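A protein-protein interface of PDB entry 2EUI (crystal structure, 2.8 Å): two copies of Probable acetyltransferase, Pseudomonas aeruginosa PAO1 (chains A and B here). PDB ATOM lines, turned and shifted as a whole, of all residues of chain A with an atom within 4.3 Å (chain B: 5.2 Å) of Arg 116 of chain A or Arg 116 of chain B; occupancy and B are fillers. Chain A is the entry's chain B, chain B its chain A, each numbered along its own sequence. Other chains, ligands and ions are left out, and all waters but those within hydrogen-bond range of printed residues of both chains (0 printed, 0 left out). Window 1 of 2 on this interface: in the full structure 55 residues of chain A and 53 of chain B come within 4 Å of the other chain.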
ATOM      1  N   TRP A  79     -15.050 -10.421  32.130  1.00  0.00           N
ATOM      2  CA  TRP A  79     -13.992 -11.193  32.760  1.00  0.00           C
ATOM      3  C   TRP A  79     -14.255 -12.666  32.583  1.00  0.00           C
ATOM      4  O   TRP A  79     -15.361 -13.141  32.835  1.00  0.00           O
ATOM      5  CB  TRP A  79     -13.845 -10.851  34.245  1.00  0.00           C
ATOM      6  CG  TRP A  79     -13.327  -9.472  34.458  1.00  0.00           C
ATOM      7  CD1 TRP A  79     -14.062  -8.354  34.709  1.00  0.00           C
ATOM      8  CD2 TRP A  79     -11.968  -9.039  34.337  1.00  0.00           C
ATOM      9  NE1 TRP A  79     -13.253  -7.248  34.745  1.00  0.00           N
ATOM     10  CE2 TRP A  79     -11.959  -7.636  34.514  1.00  0.00           C
ATOM     11  CE3 TRP A  79     -10.759  -9.695  34.086  1.00  0.00           C
ATOM     12  CZ2 TRP A  79     -10.783  -6.874  34.458  1.00  0.00           C
ATOM     13  CZ3 TRP A  79      -9.587  -8.937  34.029  1.00  0.00           C
ATOM     14  CH2 TRP A  79      -9.612  -7.538  34.212  1.00  0.00           C
ATOM     15  N   ILE A  80     -13.227 -13.380  32.135  1.00  0.00           N
ATOM     16  CA  ILE A  80     -13.319 -14.818  31.913  1.00  0.00           C
ATOM     17  C   ILE A  80     -12.559 -15.605  32.983  1.00  0.00           C
ATOM     18  O   ILE A  80     -11.322 -15.618  33.012  1.00  0.00           O
ATOM     19  CB  ILE A  80     -12.771 -15.182  30.517  1.00  0.00           C
ATOM     20  CG1 ILE A  80     -13.576 -14.431  29.449  1.00  0.00           C
ATOM     21  CG2 ILE A  80     -12.833 -16.683  30.299  1.00  0.00           C
ATOM     22  CD1 ILE A  80     -13.015 -14.550  28.050  1.00  0.00           C
ATOM     23  N   LEU A  81     -13.317 -16.237  33.873  1.00  0.00           N
ATOM     24  CA  LEU A  81     -12.751 -17.050  34.944  1.00  0.00           C
ATOM     25  C   LEU A  81     -12.195 -18.303  34.294  1.00  0.00           C
ATOM     26  O   LEU A  81     -12.931 -19.209  33.934  1.00  0.00           O
ATOM     27  CB  LEU A  81     -13.846 -17.410  35.937  1.00  0.00           C
ATOM     28  CG  LEU A  81     -13.508 -18.132  37.234  1.00  0.00           C
ATOM     29  CD1 LEU A  81     -12.396 -17.421  37.980  1.00  0.00           C
ATOM     30  CD2 LEU A  81     -14.775 -18.178  38.068  1.00  0.00           C
ATOM     31  N   MET A 115     -19.303 -12.052  33.803  1.00  0.00           N
ATOM     32  CA  MET A 115     -18.174 -12.945  34.042  1.00  0.00           C
ATOM     33  C   MET A 115     -18.581 -14.232  33.329  1.00  0.00           C
ATOM     34  O   MET A 115     -19.762 -14.540  33.257  1.00  0.00           O
ATOM     35  CB  MET A 115     -18.011 -13.259  35.532  1.00  0.00           C
ATOM     36  CG  MET A 115     -17.395 -12.173  36.384  1.00  0.00           C
ATOM     37  SD  MET A 115     -16.893 -12.899  38.122  1.00  0.00           S
ATOM     38  CE  MET A 115     -15.375 -13.935  37.532  1.00  0.00           C
ATOM     39  N   ARG A 116     -17.623 -14.980  32.806  1.00  0.00           N
ATOM     40  CA  ARG A 116     -17.932 -16.230  32.121  1.00  0.00           C
ATOM     41  C   ARG A 116     -17.071 -17.348  32.682  1.00  0.00           C
ATOM     42  O   ARG A 116     -15.969 -17.095  33.161  1.00  0.00           O
ATOM     43  CB  ARG A 116     -17.621 -16.125  30.625  1.00  0.00           C
ATOM     44  CG  ARG A 116     -18.615 -15.407  29.742  1.00  0.00           C
ATOM     45  CD  ARG A 116     -18.077 -15.420  28.310  1.00  0.00           C
ATOM     46  NE  ARG A 116     -19.006 -14.828  27.356  1.00  0.00           N
ATOM     47  CZ  ARG A 116     -20.167 -15.372  27.002  1.00  0.00           C
ATOM     48  NH1 ARG A 116     -20.552 -16.540  27.520  1.00  0.00           N
ATOM     49  NH2 ARG A 116     -20.954 -14.741  26.140  1.00  0.00           N
ATOM     50  N   VAL A 117     -17.572 -18.579  32.629  1.00  0.00           N
ATOM     51  CA  VAL A 117     -16.799 -19.746  33.065  1.00  0.00           C
ATOM     52  C   VAL A 117     -17.321 -20.981  32.352  1.00  0.00           C
ATOM     53  O   VAL A 117     -18.517 -21.075  32.061  1.00  0.00           O
ATOM     54  CB  VAL A 117     -16.882 -20.035  34.586  1.00  0.00           C
ATOM     55  CG1 VAL A 117     -15.858 -21.091  34.954  1.00  0.00           C
ATOM     56  CG2 VAL A 117     -16.597 -18.810  35.376  1.00  0.00           C
ATOM     57  N   PHE A 135     -23.327 -17.639  38.670  1.00  0.00           N
ATOM     58  CA  PHE A 135     -23.159 -18.234  37.354  1.00  0.00           C
ATOM     59  C   PHE A 135     -24.349 -19.124  37.020  1.00  0.00           C
ATOM     60  O   PHE A 135     -24.689 -20.044  37.765  1.00  0.00           O
ATOM     61  CB  PHE A 135     -21.860 -19.046  37.265  1.00  0.00           C
ATOM     62  CG  PHE A 135     -20.616 -18.200  37.159  1.00  0.00           C
ATOM     63  CD1 PHE A 135     -19.798 -17.984  38.271  1.00  0.00           C
ATOM     64  CD2 PHE A 135     -20.264 -17.616  35.952  1.00  0.00           C
ATOM     65  CE1 PHE A 135     -18.648 -17.198  38.177  1.00  0.00           C
ATOM     66  CE2 PHE A 135     -19.114 -16.825  35.844  1.00  0.00           C
ATOM     67  CZ  PHE A 135     -18.309 -16.618  36.960  1.00  0.00           C
ATOM     68  N   ASP A 138     -25.479 -20.110  30.475  1.00  0.00           N
ATOM     69  CA  ASP A 138     -25.575 -19.140  29.397  1.00  0.00           C
ATOM     70  C   ASP A 138     -26.661 -19.434  28.363  1.00  0.00           C
ATOM     71  O   ASP A 138     -26.493 -20.291  27.494  1.00  0.00           O
ATOM     72  CB  ASP A 138     -24.205 -19.028  28.723  1.00  0.00           C
ATOM     73  CG  ASP A 138     -24.229 -18.154  27.491  1.00  0.00           C
ATOM     74  OD1 ASP A 138     -24.953 -17.138  27.505  1.00  0.00           O
ATOM     75  OD2 ASP A 138     -23.510 -18.480  26.519  1.00  0.00           O
ATOM     76  N   PHE A 141     -26.142 -16.510  24.850  1.00  0.00           N
ATOM     77  CA  PHE A 141     -25.153 -16.662  23.789  1.00  0.00           C
ATOM     78  C   PHE A 141     -24.928 -18.096  23.336  1.00  0.00           C
ATOM     79  O   PHE A 141     -25.294 -19.050  24.020  1.00  0.00           O
ATOM     80  CB  PHE A 141     -23.826 -16.070  24.260  1.00  0.00           C
ATOM     81  CG  PHE A 141     -23.877 -14.586  24.488  1.00  0.00           C
ATOM     82  CD1 PHE A 141     -23.863 -13.709  23.410  1.00  0.00           C
ATOM     83  CD2 PHE A 141     -23.942 -14.064  25.773  1.00  0.00           C
ATOM     84  CE1 PHE A 141     -23.909 -12.336  23.606  1.00  0.00           C
ATOM     85  CE2 PHE A 141     -23.989 -12.687  25.981  1.00  0.00           C
ATOM     86  CZ  PHE A 141     -23.972 -11.822  24.893  1.00  0.00           C
ATOM     87  N   ASN A 143     -21.769 -20.500  21.918  1.00  0.00           N
ATOM     88  CA  ASN A 143     -20.309 -20.493  21.862  1.00  0.00           C
ATOM     89  C   ASN A 143     -19.571 -21.464  20.938  1.00  0.00           C
ATOM     90  O   ASN A 143     -19.845 -22.659  20.907  1.00  0.00           O
ATOM     91  CB  ASN A 143     -19.778 -20.616  23.289  1.00  0.00           C
ATOM     92  CG  ASN A 143     -20.367 -19.563  24.212  1.00  0.00           C
ATOM     93  OD1 ASN A 143     -21.478 -19.719  24.729  1.00  0.00           O
ATOM     94  ND2 ASN A 143     -19.634 -18.463  24.400  1.00  0.00           N
ATOM     95  N   TYR A 144     -18.604 -20.922  20.205  1.00  0.00           N
ATOM     96  CA  TYR A 144     -17.818 -21.698  19.261  1.00  0.00           C
ATOM     97  C   TYR A 144     -16.307 -21.689  19.510  1.00  0.00           C
ATOM     98  O   TYR A 144     -15.749 -20.762  20.107  1.00  0.00           O
ATOM     99  CB  TYR A 144     -18.079 -21.212  17.832  1.00  0.00           C
ATOM    100  CG  TYR A 144     -19.536 -21.168  17.450  1.00  0.00           C
ATOM    101  CD1 TYR A 144     -20.335 -20.083  17.799  1.00  0.00           C
ATOM    102  CD2 TYR A 144     -20.117 -22.214  16.737  1.00  0.00           C
ATOM    103  CE1 TYR A 144     -21.682 -20.043  17.440  1.00  0.00           C
ATOM    104  CE2 TYR A 144     -21.451 -22.184  16.377  1.00  0.00           C
ATOM    105  CZ  TYR A 144     -22.229 -21.098  16.729  1.00  0.00           C
ATOM    106  OH  TYR A 144     -23.551 -21.068  16.367  1.00  0.00           O
ATOM    107  N   VAL B  78      -4.528 -17.826  22.654  1.00  0.00           N
ATOM    108  CA  VAL B  78      -5.894 -18.094  22.214  1.00  0.00           C
ATOM    109  C   VAL B  78      -6.404 -16.765  21.671  1.00  0.00           C
ATOM    110  O   VAL B  78      -6.038 -15.702  22.183  1.00  0.00           O
ATOM    111  CB  VAL B  78      -6.838 -18.509  23.360  1.00  0.00           C
ATOM    112  CG1 VAL B  78      -8.277 -18.546  22.854  1.00  0.00           C
ATOM    113  CG2 VAL B  78      -6.445 -19.855  23.898  1.00  0.00           C
ATOM    114  N   TRP B  79      -7.236 -16.814  20.635  1.00  0.00           N
ATOM    115  CA  TRP B  79      -7.774 -15.592  20.064  1.00  0.00           C
ATOM    116  C   TRP B  79      -9.289 -15.566  20.135  1.00  0.00           C
ATOM    117  O   TRP B  79      -9.961 -16.440  19.598  1.00  0.00           O
ATOM    118  CB  TRP B  79      -7.316 -15.415  18.610  1.00  0.00           C
ATOM    119  CG  TRP B  79      -5.889 -15.012  18.498  1.00  0.00           C
ATOM    120  CD1 TRP B  79      -4.828 -15.813  18.194  1.00  0.00           C
ATOM    121  CD2 TRP B  79      -5.346 -13.723  18.784  1.00  0.00           C
ATOM    122  NE1 TRP B  79      -3.654 -15.106  18.286  1.00  0.00           N
ATOM    123  CE2 TRP B  79      -3.945 -13.816  18.655  1.00  0.00           C
ATOM    124  CE3 TRP B  79      -5.906 -12.496  19.164  1.00  0.00           C
ATOM    125  CZ2 TRP B  79      -3.094 -12.727  18.869  1.00  0.00           C
ATOM    126  CZ3 TRP B  79      -5.058 -11.413  19.378  1.00  0.00           C
ATOM    127  CH2 TRP B  79      -3.670 -11.540  19.239  1.00  0.00           C
ATOM    128  N   ILE B  80      -9.817 -14.563  20.828  1.00  0.00           N
ATOM    129  CA  ILE B  80     -11.247 -14.399  20.956  1.00  0.00           C
ATOM    130  C   ILE B  80     -11.662 -13.537  19.775  1.00  0.00           C
ATOM    131  O   ILE B  80     -11.070 -12.487  19.521  1.00  0.00           O
ATOM    132  CB  ILE B  80     -11.625 -13.657  22.249  1.00  0.00           C
ATOM    133  CG1 ILE B  80     -11.093 -14.407  23.469  1.00  0.00           C
ATOM    134  CG2 ILE B  80     -13.125 -13.518  22.342  1.00  0.00           C
ATOM    135  CD1 ILE B  80     -11.514 -13.784  24.788  1.00  0.00           C
ATOM    136  N   LEU B  81     -12.669 -13.990  19.044  1.00  0.00           N
ATOM    137  CA  LEU B  81     -13.166 -13.253  17.896  1.00  0.00           C
ATOM    138  C   LEU B  81     -14.509 -12.673  18.297  1.00  0.00           C
ATOM    139  O   LEU B  81     -15.510 -13.382  18.335  1.00  0.00           O
ATOM    140  CB  LEU B  81     -13.332 -14.200  16.712  1.00  0.00           C
ATOM    141  CG  LEU B  81     -13.796 -13.652  15.362  1.00  0.00           C
ATOM    142  CD1 LEU B  81     -12.848 -12.552  14.867  1.00  0.00           C
ATOM    143  CD2 LEU B  81     -13.844 -14.809  14.375  1.00  0.00           C
ATOM    144  N   ARG B 114      -6.186 -22.179  19.850  1.00  0.00           N
ATOM    145  CA  ARG B 114      -7.503 -22.084  19.241  1.00  0.00           C
ATOM    146  C   ARG B 114      -7.987 -20.645  19.134  1.00  0.00           C
ATOM    147  O   ARG B 114      -7.316 -19.701  19.552  1.00  0.00           O
ATOM    148  CB  ARG B 114      -8.510 -22.882  20.079  1.00  0.00           C
ATOM    149  CG  ARG B 114      -8.765 -22.282  21.463  1.00  0.00           C
ATOM    150  CD  ARG B 114      -9.638 -23.175  22.315  1.00  0.00           C
ATOM    151  NE  ARG B 114      -8.979 -24.447  22.572  1.00  0.00           N
ATOM    152  CZ  ARG B 114      -8.302 -24.743  23.678  1.00  0.00           C
ATOM    153  NH1 ARG B 114      -8.197 -23.855  24.660  1.00  0.00           N
ATOM    154  NH2 ARG B 114      -7.711 -25.926  23.787  1.00  0.00           N
ATOM    155  N   MET B 115      -9.165 -20.510  18.549  1.00  0.00           N
ATOM    156  CA  MET B 115      -9.834 -19.243  18.391  1.00  0.00           C
ATOM    157  C   MET B 115     -11.183 -19.563  18.993  1.00  0.00           C
ATOM    158  O   MET B 115     -11.714 -20.656  18.783  1.00  0.00           O
ATOM    159  CB  MET B 115     -10.009 -18.882  16.921  1.00  0.00           C
ATOM    160  CG  MET B 115      -8.796 -18.276  16.247  1.00  0.00           C
ATOM    161  SD  MET B 115      -9.276 -17.706  14.458  1.00  0.00           S
ATOM    162  CE  MET B 115      -9.701 -15.853  14.815  1.00  0.00           C
ATOM    163  N   ARG B 116     -11.727 -18.623  19.751  1.00  0.00           N
ATOM    164  CA  ARG B 116     -13.015 -18.813  20.393  1.00  0.00           C
ATOM    165  C   ARG B 116     -13.909 -17.631  20.028  1.00  0.00           C
ATOM    166  O   ARG B 116     -13.470 -16.482  20.027  1.00  0.00           O
ATOM    167  CB  ARG B 116     -12.803 -18.921  21.911  1.00  0.00           C
ATOM    168  CG  ARG B 116     -14.066 -18.963  22.765  1.00  0.00           C
ATOM    169  CD  ARG B 116     -14.674 -17.561  22.985  1.00  0.00           C
ATOM    170  NE  ARG B 116     -15.691 -17.536  24.042  1.00  0.00           N
ATOM    171  CZ  ARG B 116     -15.445 -17.791  25.331  1.00  0.00           C
ATOM    172  NH1 ARG B 116     -14.211 -18.095  25.737  1.00  0.00           N
ATOM    173  NH2 ARG B 116     -16.434 -17.738  26.220  1.00  0.00           N
ATOM    174  N   VAL B 117     -15.159 -17.920  19.692  1.00  0.00           N
ATOM    175  CA  VAL B 117     -16.104 -16.873  19.339  1.00  0.00           C
ATOM    176  C   VAL B 117     -17.388 -17.054  20.141  1.00  0.00           C
ATOM    177  O   VAL B 117     -17.779 -18.168  20.471  1.00  0.00           O
ATOM    178  CB  VAL B 117     -16.440 -16.893  17.815  1.00  0.00           C
ATOM    179  CG1 VAL B 117     -17.225 -18.133  17.474  1.00  0.00           C
ATOM    180  CG2 VAL B 117     -17.231 -15.659  17.435  1.00  0.00           C
ATOM    181  N   SER B 118     -18.041 -15.946  20.460  1.00  0.00           N
ATOM    182  CA  SER B 118     -19.278 -15.992  21.219  1.00  0.00           C
ATOM    183  C   SER B 118     -20.229 -15.000  20.568  1.00  0.00           C
ATOM    184  O   SER B 118     -19.832 -13.874  20.267  1.00  0.00           O
ATOM    185  CB  SER B 118     -18.999 -15.603  22.672  1.00  0.00           C
ATOM    186  OG  SER B 118     -20.145 -15.777  23.474  1.00  0.00           O
ATOM    187  N   PHE B 135     -15.278 -22.771  12.933  1.00  0.00           N
ATOM    188  CA  PHE B 135     -15.940 -22.812  14.236  1.00  0.00           C
ATOM    189  C   PHE B 135     -16.983 -23.903  14.470  1.00  0.00           C
ATOM    190  O   PHE B 135     -17.816 -24.185  13.609  1.00  0.00           O
ATOM    191  CB  PHE B 135     -16.573 -21.454  14.546  1.00  0.00           C
ATOM    192  CG  PHE B 135     -15.581 -20.400  14.918  1.00  0.00           C
ATOM    193  CD1 PHE B 135     -15.169 -19.452  13.985  1.00  0.00           C
ATOM    194  CD2 PHE B 135     -15.030 -20.377  16.200  1.00  0.00           C
ATOM    195  CE1 PHE B 135     -14.215 -18.495  14.322  1.00  0.00           C
ATOM    196  CE2 PHE B 135     -14.078 -19.433  16.555  1.00  0.00           C
ATOM    197  CZ  PHE B 135     -13.666 -18.489  15.618  1.00  0.00           C
ATOM    198  N   TYR B 144     -21.150 -20.926  31.473  1.00  0.00           N
ATOM    199  CA  TYR B 144     -21.814 -20.090  32.464  1.00  0.00           C
ATOM    200  C   TYR B 144     -21.702 -18.586  32.250  1.00  0.00           C
ATOM    201  O   TYR B 144     -20.800 -18.091  31.576  1.00  0.00           O
ATOM    202  CB  TYR B 144     -21.303 -20.432  33.859  1.00  0.00           C
ATOM    203  CG  TYR B 144     -21.831 -21.742  34.376  1.00  0.00           C
ATOM    204  CD1 TYR B 144     -21.268 -22.952  33.970  1.00  0.00           C
ATOM    205  CD2 TYR B 144     -22.918 -21.775  35.253  1.00  0.00           C
ATOM    206  CE1 TYR B 144     -21.773 -24.166  34.424  1.00  0.00           C
ATOM    207  CE2 TYR B 144     -23.433 -22.981  35.710  1.00  0.00           C
ATOM    208  CZ  TYR B 144     -22.855 -24.172  35.294  1.00  0.00           C
ATOM    209  OH  TYR B 144     -23.355 -25.362  35.757  1.00  0.00           O
ATOM    210  N   THR B 145     -22.633 -17.864  32.853  1.00  0.00           N
ATOM    211  CA  THR B 145     -22.664 -16.418  32.750  1.00  0.00           C
ATOM    212  C   THR B 145     -23.192 -15.818  34.032  1.00  0.00           C
ATOM    213  O   THR B 145     -24.161 -16.307  34.593  1.00  0.00           O
ATOM    214  CB  THR B 145     -23.569 -15.972  31.580  1.00  0.00           C
ATOM    215  OG1 THR B 145     -22.792 -15.939  30.378  1.00  0.00           O
ATOM    216  CG2 THR B 145     -24.172 -14.596  31.838  1.00  0.00           C
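Met 115 of chain A touches Thr 145 of chain B. Arg 116 of chain B touches Arg 116 of chain A. O of Tyr 144 of chain B touches CA of Arg 116 of chain A (3.5 Å). OG1 of Thr 145 of chain B touches NH1 of Arg 116 of chain A, at 3.7 Å. Phe 135 of chain A touches Tyr 144 of chain B (C to CD2, 3.5 Å). OG1 of Thr 145 of chain B touches CB of Asp 138 of chain A, 3.8 Å away. ND2 of Asn 143 of chain A touches NH2 of Arg 116 of chain B (3.8 Å). O of Val 117 of chain B touches CA of Asn 143 of chain A, 3.7 Å away. Arg 116 of chain B touches Tyr 144 of chain A. Tyr 144 of chain A touches Phe 135 of chain B.
Of chain B, only Arg 116, Ser 118, Tyr 144 and Thr 145 come within 4 Å of Arg 116 of chain A. Printed residues of chain B within 4 Å of Val 117 of chain A: Tyr 144. Printed residues of chain B within 4 Å of Phe 135 of chain A: Tyr 144 (3.5 Å) and Thr 145 (3.5 Å). Met 115 of chain B touches none of the printed residues of chain A. Of the printed residues of chain A, Arg 116 of chain B touches Arg 116, Asn 143 and Tyr 144. Printed residues of chain A within 4 Å of Phe 135 of chain B: Tyr 144 (3.6 Å). Printed residues of chain A within 4 Å of Thr 145 of chain B: Met 115, Arg 116, Phe 135 and Asp 138. The nearest printed residue of chain B that does not touch Arg 116 of chain A is Val 117 of chain B (7.3 Å). The nearest printed residue of chain A that does not touch Ile 80 of chain B is Arg 116 of chain A (7.6 Å).
The backbone carbonyl oxygen (O) of Val 117 of chain B lies within hydrogen-bond range of the backbone NH (N) of Tyr 144 of chain A (2.9 Å). The guanidinium group of Arg 116 of chain A sits at hydrogen-bond distance from the side-chain hydroxyl of Ser 118 of chain B. OG of Ser 118 of chain B lies within hydrogen-bond range of ND2 of Asn 143 of chain A (2.9 Å). N of Tyr 144 of chain B sits at hydrogen-bond distance from O of Val 117 of chain A (2.7 Å).
Hydrophobic or aromatic side chains of chain A within 4 Å of the printed part of chain B: Ile 80, Phe 135, Phe 141 and Tyr 144. Of the 12 printed residues of chain B, 7 touch a printed residue of chain A. Hydrophobic or aromatic side chains of chain B that line the printed part of chain A: Ile 80, Val 117, Phe 135 and Tyr 144. Among the printed residues, no Asp or Glu carboxylate lies within 4 Å of a Lys or Arg side-chain nitrogen of the other chain.
Ile 80 of chain B touches its own counterpart, Ile 80 of chain A. Arg 116 of chain A touches Tyr 144 of chain B, and with the chains exchanged Tyr 144 of chain A touches Arg 116 of chain B. Val 117 of chain A touches Tyr 144 of chain B, and with the chains exchanged Tyr 144 of chain A touches Val 117 of chain B. Phe 135 of chain A touches Tyr 144 of chain B, and with the chains exchanged Tyr 144 of chain A touches Phe 135 of chain B. Of the 17 pairs that touch across the chains among the printed residues, 8 have their exchanged pair printed and touching as well.
O of Trp 79 of chain B sits at hydrogen-bond distance from N of Arg 116 of chain B (2.8 Å). The backbone NH of Leu 81 of chain B lies within hydrogen-bond range of the backbone carbonyl oxygen of Arg 116 of chain B, 2.8 Å away. O of Trp 79 of chain A is in hydrogen-bond range of N of Arg 116 of chain A (2.9 Å). The backbone NH of Leu 81 of chain A sits at hydrogen-bond distance from the backbone carbonyl oxygen of Arg 116 of chain A (2.9 Å). NH1 of Arg 116 of chain A is in salt-bridge range of OD2 of Asp 138 of chain A, at 3.7 Å. The side-chain carboxylate (OD1) of Asp 138 of chain A lies within hydrogen-bond range of the backbone NH (N) of Phe 141 of chain A (3.0 Å).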
